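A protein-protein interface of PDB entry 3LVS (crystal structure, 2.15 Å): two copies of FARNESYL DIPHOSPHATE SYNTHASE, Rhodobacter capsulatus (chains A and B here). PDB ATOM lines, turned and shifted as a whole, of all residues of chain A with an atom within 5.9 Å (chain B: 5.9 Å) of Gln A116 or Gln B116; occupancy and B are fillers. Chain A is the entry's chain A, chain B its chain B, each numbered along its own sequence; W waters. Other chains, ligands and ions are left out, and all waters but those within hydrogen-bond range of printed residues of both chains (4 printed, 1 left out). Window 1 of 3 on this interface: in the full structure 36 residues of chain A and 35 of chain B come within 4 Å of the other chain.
The side-chain amide nitrogen (NE2) of Gln B116 sits close to the side-chain amide nitrogen (NE2) of Gln A116 (3.4 Å). The side-chain amide oxygen of Gln A116 sits at hydrogen-bond distance from the side-chain hydroxyl of Thr B117 (2.7 Å). O of Asp A113 sits at hydrogen-bond distance from NE2 of Gln B116. OG1 of Thr A117 lies within hydrogen-bond range of OE1 of Gln B116 (2.5 Å). NE2 of Gln A116 sits at hydrogen-bond distance from O of Asp B113 (3.1 Å).
OG1 of Thr A117 lies within hydrogen-bond range of O of Asp A113 (2.9 Å). The side-chain hydroxyl of Tyr B77 sits close to the side-chain amide nitrogen of Gln B116 (3.4 Å). The side-chain amide nitrogen (NE2) of Gln A116 sits at hydrogen-bond distance from the side-chain hydroxyl (OH) of Tyr A77. The backbone carbonyl oxygen (O) of Asp B113 is in hydrogen-bond range of the side-chain hydroxyl (OG1) of Thr B117 (2.8 Å). The side-chain hydroxyl of Thr B117 sits close to the backbone carbonyl oxygen of Ala B114, at 3.5 Å.
Among the printed residues, pairs that only touch across the chains: Asp A113 with Tyr B77 (3.2 Å), Tyr A77 with Asp B113 (3.2 Å), Phe A120 with Phe B120 (3.5 Å), Asp A113 with Asp B113 (3.6 Å), Phe A120 with Thr B117 (3.8 Å), Ser A145 with Thr B117 (3.9 Å) and Thr A117 with Phe B120 (3.9 Å).
Printed residues of chain B within 4 Å of Tyr A77: Asp B113 (3.2 Å). Ala A114 touches none of the printed residues of chain B. Printed residues of chain B within 4 Å of Gln A116: Asp B113, Gln B116 and Thr B117. Of the printed residues of chain A, Asp B113 touches Tyr A77, Asp A113 and Gln A116. Gln B116 touches just these residues of chain A: Asp A113, Gln A116 and Thr A117. Leu B118 touches none of the printed residues of chain A. The nearest printed residue of chain A that does not touch Phe B120 is Gln A116 (5.3 Å).
Of the 15 printed residues of chain A, 6 touch a printed residue of chain B. Hydrophobic or aromatic side chains of chain A that line the printed part of chain B: Tyr A77 and Phe A120. Hydrophobic or aromatic side chains of chain B within 4 Å of the printed part of chain A: Tyr B77 and Phe B120. Among the printed residues, 12 pairs touch across the chains.
Tyr A77 touches Asp B113, and with the chains exchanged Asp A113 touches Tyr B77. Asp A113 touches Gln B116, and with the chains exchanged Gln A116 touches Asp B113. Gln B116 touches its own counterpart, Gln A116. Gln A116 touches Thr B117, and with the chains exchanged Thr A117 touches Gln B116. Positions printed for both chains: 73, 74, 77, 111, 112, 113, 114, 115, 116, 117, 118, 119, 120, 121 and 145.
Water W3 lies within hydrogen-bond range of OH of Tyr A77 (2.5 Å), O of Ser A145 (2.7 Å) and OG1 of Thr B117 (3.0 Å). Water W4 lies within hydrogen-bond range of the side-chain carboxylate (OD2) of Asp A113 (2.7 Å) and the side-chain hydroxyl (OH) of Tyr B77 (3.2 Å). Water W1 lies within hydrogen-bond range of NE2 of Gln B116 (2.7 Å), OD1 of Asp A113 (2.8 Å), OD1 of Asp B113 (2.8 Å) and NE2 of Gln A116 (3.2 Å). Water W2 bridges OD2 of Asp B113 (3.0 Å) and OH of Tyr A77 (3.2 Å).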
ATOM      1  N   ALA A  73      15.967  -8.515 -10.068  1.00  0.00           N
ATOM      2  CA  ALA A  73      16.439  -9.713 -10.754  1.00  0.00           C
ATOM      3  C   ALA A  73      17.949  -9.703 -10.819  1.00  0.00           C
ATOM      4  O   ALA A  73      18.584 -10.733 -10.588  1.00  0.00           O
ATOM      5  CB  ALA A  73      15.831  -9.833 -12.168  1.00  0.00           C
ATOM      6  N   LEU A  74      18.520  -8.531 -11.104  1.00  0.00           N
ATOM      7  CA  LEU A  74      19.967  -8.378 -11.139  1.00  0.00           C
ATOM      8  C   LEU A  74      20.585  -8.607  -9.760  1.00  0.00           C
ATOM      9  O   LEU A  74      21.600  -9.299  -9.629  1.00  0.00           O
ATOM     10  CB  LEU A  74      20.374  -7.008 -11.708  1.00  0.00           C
ATOM     11  CG  LEU A  74      21.806  -7.229 -12.224  1.00  0.00           C
ATOM     12  CD1 LEU A  74      21.981  -6.902 -13.689  1.00  0.00           C
ATOM     13  CD2 LEU A  74      22.856  -6.611 -11.326  1.00  0.00           C
ATOM     14  N   TYR A  77      20.439 -12.356  -8.954  1.00  0.00           N
ATOM     15  CA  TYR A  77      21.506 -13.011  -9.694  1.00  0.00           C
ATOM     16  C   TYR A  77      22.822 -12.905  -8.933  1.00  0.00           C
ATOM     17  O   TYR A  77      23.504 -13.914  -8.740  1.00  0.00           O
ATOM     18  CB  TYR A  77      21.596 -12.448 -11.141  1.00  0.00           C
ATOM     19  CG  TYR A  77      22.962 -11.958 -11.606  1.00  0.00           C
ATOM     20  CD1 TYR A  77      24.043 -12.830 -11.764  1.00  0.00           C
ATOM     21  CD2 TYR A  77      23.158 -10.616 -11.906  1.00  0.00           C
ATOM     22  CE1 TYR A  77      25.293 -12.353 -12.165  1.00  0.00           C
ATOM     23  CE2 TYR A  77      24.383 -10.133 -12.312  1.00  0.00           C
ATOM     24  CZ  TYR A  77      25.444 -11.000 -12.439  1.00  0.00           C
ATOM     25  OH  TYR A  77      26.645 -10.503 -12.855  1.00  0.00           O
ATOM     26  N   ALA A 111      21.077 -20.434 -12.933  1.00  0.00           N
ATOM     27  CA  ALA A 111      19.969 -19.591 -12.452  1.00  0.00           C
ATOM     28  C   ALA A 111      20.459 -18.157 -12.282  1.00  0.00           C
ATOM     29  O   ALA A 111      19.700 -17.219 -12.480  1.00  0.00           O
ATOM     30  CB  ALA A 111      19.390 -20.121 -11.162  1.00  0.00           C
ATOM     31  N   GLY A 112      21.744 -18.009 -11.948  1.00  0.00           N
ATOM     32  CA  GLY A 112      22.376 -16.699 -11.877  1.00  0.00           C
ATOM     33  C   GLY A 112      22.394 -16.017 -13.228  1.00  0.00           C
ATOM     34  O   GLY A 112      21.742 -14.975 -13.405  1.00  0.00           O
ATOM     35  N   ASP A 113      23.129 -16.623 -14.179  1.00  0.00           N
ATOM     36  CA  ASP A 113      23.094 -16.234 -15.580  1.00  0.00           C
ATOM     37  C   ASP A 113      21.730 -15.839 -16.181  1.00  0.00           C
ATOM     38  O   ASP A 113      21.638 -14.804 -16.841  1.00  0.00           O
ATOM     39  CB  ASP A 113      23.618 -17.380 -16.392  1.00  0.00           C
ATOM     40  CG  ASP A 113      25.081 -17.653 -16.097  1.00  0.00           C
ATOM     41  OD1 ASP A 113      25.718 -16.794 -15.443  1.00  0.00           O
ATOM     42  OD2 ASP A 113      25.582 -18.717 -16.495  1.00  0.00           O
ATOM     43  N   ALA A 114      20.704 -16.659 -15.968  1.00  0.00           N
ATOM     44  CA  ALA A 114      19.396 -16.406 -16.577  1.00  0.00           C
ATOM     45  C   ALA A 114      18.702 -15.230 -15.912  1.00  0.00           C
ATOM     46  O   ALA A 114      17.953 -14.503 -16.558  1.00  0.00           O
ATOM     47  CB  ALA A 114      18.528 -17.647 -16.510  1.00  0.00           C
ATOM     48  N   LEU A 115      18.953 -15.061 -14.617  1.00  0.00           N
ATOM     49  CA  LEU A 115      18.501 -13.901 -13.865  1.00  0.00           C
ATOM     50  C   LEU A 115      19.105 -12.578 -14.348  1.00  0.00           C
ATOM     51  O   LEU A 115      18.383 -11.579 -14.441  1.00  0.00           O
ATOM     52  CB  LEU A 115      18.717 -14.108 -12.366  1.00  0.00           C
ATOM     53  CG  LEU A 115      17.566 -14.831 -11.659  1.00  0.00           C
ATOM     54  CD1 LEU A 115      17.993 -15.198 -10.238  1.00  0.00           C
ATOM     55  CD2 LEU A 115      16.275 -13.989 -11.661  1.00  0.00           C
ATOM     56  N   GLN A 116      20.401 -12.573 -14.686  1.00  0.00           N
ATOM     57  CA  GLN A 116      20.996 -11.397 -15.312  1.00  0.00           C
ATOM     58  C   GLN A 116      20.363 -11.138 -16.675  1.00  0.00           C
ATOM     59  O   GLN A 116      19.999  -9.989 -16.976  1.00  0.00           O
ATOM     60  CB  GLN A 116      22.537 -11.464 -15.449  1.00  0.00           C
ATOM     61  CG  GLN A 116      23.044 -10.176 -16.082  1.00  0.00           C
ATOM     62  CD  GLN A 116      24.545 -10.059 -16.308  1.00  0.00           C
ATOM     63  OE1 GLN A 116      25.004  -9.007 -16.738  1.00  0.00           O
ATOM     64  NE2 GLN A 116      25.303 -11.108 -16.028  1.00  0.00           N
ATOM     65  N   THR A 117      20.201 -12.201 -17.473  1.00  0.00           N
ATOM     66  CA  THR A 117      19.585 -12.073 -18.793  1.00  0.00           C
ATOM     67  C   THR A 117      18.129 -11.527 -18.667  1.00  0.00           C
ATOM     68  O   THR A 117      17.719 -10.668 -19.437  1.00  0.00           O
ATOM     69  CB  THR A 117      19.551 -13.379 -19.582  1.00  0.00           C
ATOM     70  OG1 THR A 117      20.852 -14.030 -19.568  1.00  0.00           O
ATOM     71  CG2 THR A 117      19.207 -13.049 -21.017  1.00  0.00           C
ATOM     72  N   LEU A 118      17.396 -12.028 -17.690  1.00  0.00           N
ATOM     73  CA  LEU A 118      16.000 -11.578 -17.453  1.00  0.00           C
ATOM     74  C   LEU A 118      15.940 -10.092 -17.063  1.00  0.00           C
ATOM     75  O   LEU A 118      15.058  -9.353 -17.509  1.00  0.00           O
ATOM     76  CB  LEU A 118      15.357 -12.451 -16.372  1.00  0.00           C
ATOM     77  CG  LEU A 118      13.972 -12.032 -15.828  1.00  0.00           C
ATOM     78  CD1 LEU A 118      12.882 -12.373 -16.825  1.00  0.00           C
ATOM     79  CD2 LEU A 118      13.705 -12.703 -14.510  1.00  0.00           C
ATOM     80  N   ALA A 119      16.905  -9.662 -16.250  1.00  0.00           N
ATOM     81  CA  ALA A 119      17.021  -8.269 -15.831  1.00  0.00           C
ATOM     82  C   ALA A 119      17.076  -7.315 -17.030  1.00  0.00           C
ATOM     83  O   ALA A 119      16.334  -6.324 -17.078  1.00  0.00           O
ATOM     84  CB  ALA A 119      18.241  -8.080 -14.925  1.00  0.00           C
ATOM     85  N   PHE A 120      17.934  -7.630 -18.000  1.00  0.00           N
ATOM     86  CA  PHE A 120      18.018  -6.843 -19.235  1.00  0.00           C
ATOM     87  C   PHE A 120      16.818  -6.972 -20.161  1.00  0.00           C
ATOM     88  O   PHE A 120      16.459  -5.989 -20.822  1.00  0.00           O
ATOM     89  CB  PHE A 120      19.289  -7.143 -20.004  1.00  0.00           C
ATOM     90  CG  PHE A 120      20.499  -6.618 -19.344  1.00  0.00           C
ATOM     91  CD1 PHE A 120      21.414  -7.487 -18.746  1.00  0.00           C
ATOM     92  CD2 PHE A 120      20.730  -5.247 -19.289  1.00  0.00           C
ATOM     93  CE1 PHE A 120      22.544  -6.993 -18.108  1.00  0.00           C
ATOM     94  CE2 PHE A 120      21.857  -4.738 -18.654  1.00  0.00           C
ATOM     95  CZ  PHE A 120      22.773  -5.613 -18.065  1.00  0.00           C
ATOM     96  N   GLU A 121      16.210  -8.164 -20.210  1.00  0.00           N
ATOM     97  CA  GLU A 121      14.953  -8.347 -20.941  1.00  0.00           C
ATOM     98  C   GLU A 121      13.847  -7.451 -20.390  1.00  0.00           C
ATOM     99  O   GLU A 121      13.067  -6.895 -21.159  1.00  0.00           O
ATOM    100  CB  GLU A 121      14.478  -9.806 -20.925  1.00  0.00           C
ATOM    101  CG  GLU A 121      13.296 -10.074 -21.892  1.00  0.00           C
ATOM    102  CD  GLU A 121      12.881 -11.540 -21.983  1.00  0.00           C
ATOM    103  OE1 GLU A 121      12.771 -12.055 -23.120  1.00  0.00           O
ATOM    104  OE2 GLU A 121      12.667 -12.183 -20.930  1.00  0.00           O
ATOM    105  N   SER A 145      26.231  -2.752 -13.391  1.00  0.00           N
ATOM    106  CA  SER A 145      26.338  -4.188 -13.111  1.00  0.00           C
ATOM    107  C   SER A 145      27.649  -4.860 -13.501  1.00  0.00           C
ATOM    108  O   SER A 145      27.980  -5.897 -12.949  1.00  0.00           O
ATOM    109  CB  SER A 145      25.187  -4.929 -13.778  1.00  0.00           C
ATOM    110  OG  SER A 145      23.949  -4.327 -13.395  1.00  0.00           O
ATOM    111  N   ALA B  73      30.764 -11.733 -27.322  1.00  0.00           N
ATOM    112  CA  ALA B  73      30.983 -11.565 -25.887  1.00  0.00           C
ATOM    113  C   ALA B  73      30.132 -12.591 -25.160  1.00  0.00           C
ATOM    114  O   ALA B  73      30.613 -13.286 -24.254  1.00  0.00           O
ATOM    115  CB  ALA B  73      30.617 -10.144 -25.422  1.00  0.00           C
ATOM    116  N   LEU B  74      28.879 -12.696 -25.603  1.00  0.00           N
ATOM    117  CA  LEU B  74      27.936 -13.651 -25.063  1.00  0.00           C
ATOM    118  C   LEU B  74      28.316 -15.105 -25.306  1.00  0.00           C
ATOM    119  O   LEU B  74      28.115 -15.931 -24.413  1.00  0.00           O
ATOM    120  CB  LEU B  74      26.555 -13.402 -25.624  1.00  0.00           C
ATOM    121  CG  LEU B  74      25.578 -13.759 -24.513  1.00  0.00           C
ATOM    122  CD1 LEU B  74      24.507 -12.710 -24.380  1.00  0.00           C
ATOM    123  CD2 LEU B  74      25.006 -15.168 -24.677  1.00  0.00           C
ATOM    124  N   TYR B  77      31.131 -15.593 -22.938  1.00  0.00           N
ATOM    125  CA  TYR B  77      30.725 -15.756 -21.563  1.00  0.00           C
ATOM    126  C   TYR B  77      30.233 -17.161 -21.283  1.00  0.00           C
ATOM    127  O   TYR B  77      30.393 -17.665 -20.162  1.00  0.00           O
ATOM    128  CB  TYR B  77      29.666 -14.709 -21.183  1.00  0.00           C
ATOM    129  CG  TYR B  77      28.363 -15.292 -20.745  1.00  0.00           C
ATOM    130  CD1 TYR B  77      28.291 -16.220 -19.669  1.00  0.00           C
ATOM    131  CD2 TYR B  77      27.167 -14.816 -21.288  1.00  0.00           C
ATOM    132  CE1 TYR B  77      27.061 -16.724 -19.206  1.00  0.00           C
ATOM    133  CE2 TYR B  77      25.947 -15.297 -20.843  1.00  0.00           C
ATOM    134  CZ  TYR B  77      25.880 -16.230 -19.771  1.00  0.00           C
ATOM    135  OH  TYR B  77      24.686 -16.779 -19.358  1.00  0.00           O
ATOM    136  N   ALA B 111      34.268 -13.271 -14.563  1.00  0.00           N
ATOM    137  CA  ALA B 111      34.573 -12.944 -15.952  1.00  0.00           C
ATOM    138  C   ALA B 111      33.382 -13.223 -16.880  1.00  0.00           C
ATOM    139  O   ALA B 111      33.101 -12.419 -17.767  1.00  0.00           O
ATOM    140  CB  ALA B 111      35.816 -13.686 -16.431  1.00  0.00           C
ATOM    141  N   GLY B 112      32.686 -14.340 -16.652  1.00  0.00           N
ATOM    142  CA  GLY B 112      31.519 -14.703 -17.440  1.00  0.00           C
ATOM    143  C   GLY B 112      30.321 -13.826 -17.149  1.00  0.00           C
ATOM    144  O   GLY B 112      29.566 -13.497 -18.053  1.00  0.00           O
ATOM    145  N   ASP B 113      30.143 -13.452 -15.886  1.00  0.00           N
ATOM    146  CA  ASP B 113      29.099 -12.498 -15.503  1.00  0.00           C
ATOM    147  C   ASP B 113      29.251 -11.136 -16.171  1.00  0.00           C
ATOM    148  O   ASP B 113      28.268 -10.563 -16.644  1.00  0.00           O
ATOM    149  CB  ASP B 113      29.088 -12.313 -13.991  1.00  0.00           C
ATOM    150  CG  ASP B 113      28.552 -13.518 -13.271  1.00  0.00           C
ATOM    151  OD1 ASP B 113      27.753 -14.246 -13.890  1.00  0.00           O
ATOM    152  OD2 ASP B 113      28.941 -13.746 -12.101  1.00  0.00           O
ATOM    153  N   ALA B 114      30.485 -10.634 -16.185  1.00  0.00           N
ATOM    154  CA  ALA B 114      30.819  -9.319 -16.732  1.00  0.00           C
ATOM    155  C   ALA B 114      30.745  -9.309 -18.255  1.00  0.00           C
ATOM    156  O   ALA B 114      30.209  -8.357 -18.828  1.00  0.00           O
ATOM    157  CB  ALA B 114      32.203  -8.884 -16.267  1.00  0.00           C
ATOM    158  N   LEU B 115      31.295 -10.353 -18.891  1.00  0.00           N
ATOM    159  CA  LEU B 115      31.084 -10.616 -20.329  1.00  0.00           C
ATOM    160  C   LEU B 115      29.617 -10.640 -20.767  1.00  0.00           C
ATOM    161  O   LEU B 115      29.291 -10.118 -21.829  1.00  0.00           O
ATOM    162  CB  LEU B 115      31.777 -11.899 -20.788  1.00  0.00           C
ATOM    163  CG  LEU B 115      33.290 -11.796 -21.037  1.00  0.00           C
ATOM    164  CD1 LEU B 115      33.902 -13.170 -21.273  1.00  0.00           C
ATOM    165  CD2 LEU B 115      33.593 -10.858 -22.204  1.00  0.00           C
ATOM    166  N   GLN B 116      28.737 -11.219 -19.958  1.00  0.00           N
ATOM    167  CA  GLN B 116      27.307 -11.108 -20.260  1.00  0.00           C
ATOM    168  C   GLN B 116      26.877  -9.656 -20.250  1.00  0.00           C
ATOM    169  O   GLN B 116      26.216  -9.209 -21.184  1.00  0.00           O
ATOM    170  CB  GLN B 116      26.405 -11.912 -19.317  1.00  0.00           C
ATOM    171  CG  GLN B 116      24.921 -11.879 -19.821  1.00  0.00           C
ATOM    172  CD  GLN B 116      23.938 -12.698 -19.016  1.00  0.00           C
ATOM    173  OE1 GLN B 116      22.715 -12.485 -19.103  1.00  0.00           O
ATOM    174  NE2 GLN B 116      24.446 -13.624 -18.214  1.00  0.00           N
ATOM    175  N   THR B 117      27.263  -8.928 -19.203  1.00  0.00           N
ATOM    176  CA  THR B 117      26.918  -7.513 -19.078  1.00  0.00           C
ATOM    177  C   THR B 117      27.455  -6.684 -20.227  1.00  0.00           C
ATOM    178  O   THR B 117      26.739  -5.844 -20.750  1.00  0.00           O
ATOM    179  CB  THR B 117      27.408  -6.899 -17.761  1.00  0.00           C
ATOM    180  OG1 THR B 117      27.455  -7.914 -16.756  1.00  0.00           O
ATOM    181  CG2 THR B 117      26.441  -5.813 -17.310  1.00  0.00           C
ATOM    182  N   LEU B 118      28.708  -6.935 -20.609  1.00  0.00           N
ATOM    183  CA  LEU B 118      29.344  -6.250 -21.725  1.00  0.00           C
ATOM    184  C   LEU B 118      28.558  -6.422 -23.048  1.00  0.00           C
ATOM    185  O   LEU B 118      28.381  -5.464 -23.806  1.00  0.00           O
ATOM    186  CB  LEU B 118      30.798  -6.727 -21.880  1.00  0.00           C
ATOM    187  CG  LEU B 118      31.609  -6.133 -23.028  1.00  0.00           C
ATOM    188  CD1 LEU B 118      31.748  -4.625 -22.832  1.00  0.00           C
ATOM    189  CD2 LEU B 118      32.982  -6.800 -23.163  1.00  0.00           C
ATOM    190  N   ALA B 119      28.066  -7.634 -23.289  1.00  0.00           N
ATOM    191  CA  ALA B 119      27.275  -7.946 -24.484  1.00  0.00           C
ATOM    192  C   ALA B 119      26.017  -7.069 -24.601  1.00  0.00           C
ATOM    193  O   ALA B 119      25.734  -6.517 -25.679  1.00  0.00           O
ATOM    194  CB  ALA B 119      26.915  -9.402 -24.489  1.00  0.00           C
ATOM    195  N   PHE B 120      25.286  -6.919 -23.498  1.00  0.00           N
ATOM    196  CA  PHE B 120      24.105  -6.038 -23.494  1.00  0.00           C
ATOM    197  C   PHE B 120      24.414  -4.545 -23.588  1.00  0.00           C
ATOM    198  O   PHE B 120      23.647  -3.801 -24.201  1.00  0.00           O
ATOM    199  CB  PHE B 120      23.224  -6.314 -22.289  1.00  0.00           C
ATOM    200  CG  PHE B 120      22.510  -7.616 -22.372  1.00  0.00           C
ATOM    201  CD1 PHE B 120      22.982  -8.726 -21.680  1.00  0.00           C
ATOM    202  CD2 PHE B 120      21.376  -7.746 -23.164  1.00  0.00           C
ATOM    203  CE1 PHE B 120      22.312  -9.951 -21.756  1.00  0.00           C
ATOM    204  CE2 PHE B 120      20.702  -8.958 -23.254  1.00  0.00           C
ATOM    205  CZ  PHE B 120      21.173 -10.067 -22.548  1.00  0.00           C
ATOM    206  N   GLU B 121      25.518  -4.116 -22.972  1.00  0.00           N
ATOM    207  CA  GLU B 121      25.974  -2.726 -23.046  1.00  0.00           C
ATOM    208  C   GLU B 121      26.316  -2.337 -24.483  1.00  0.00           C
ATOM    209  O   GLU B 121      25.908  -1.259 -24.958  1.00  0.00           O
ATOM    210  CB  GLU B 121      27.202  -2.500 -22.162  1.00  0.00           C
ATOM    211  CG  GLU B 121      27.735  -1.067 -22.201  1.00  0.00           C
ATOM    212  CD  GLU B 121      28.574  -0.711 -20.993  1.00  0.00           C
ATOM    213  OE1 GLU B 121      28.234   0.289 -20.320  1.00  0.00           O
ATOM    214  OE2 GLU B 121      29.562  -1.427 -20.707  1.00  0.00           O
ATOM    215  N   SER B 145      19.399 -15.751 -25.108  1.00  0.00           N
ATOM    216  CA  SER B 145      20.414 -16.163 -24.149  1.00  0.00           C
ATOM    217  C   SER B 145      19.911 -16.723 -22.836  1.00  0.00           C
ATOM    218  O   SER B 145      20.646 -17.433 -22.172  1.00  0.00           O
ATOM    219  CB  SER B 145      21.388 -15.015 -23.879  1.00  0.00           C
ATOM    220  OG  SER B 145      21.884 -14.503 -25.109  1.00  0.00           O
HETATM  221  O   HOH W   1      26.200 -14.166 -16.193  1.00  0.00           O
HETATM  222  O   HOH W   2      28.462 -11.379 -10.349  1.00  0.00           O
HETATM  223  O   HOH W   3      26.761  -8.192 -13.822  1.00  0.00           O
HETATM  224  O   HOH W   4      25.334 -19.849 -18.930  1.00  0.00           O
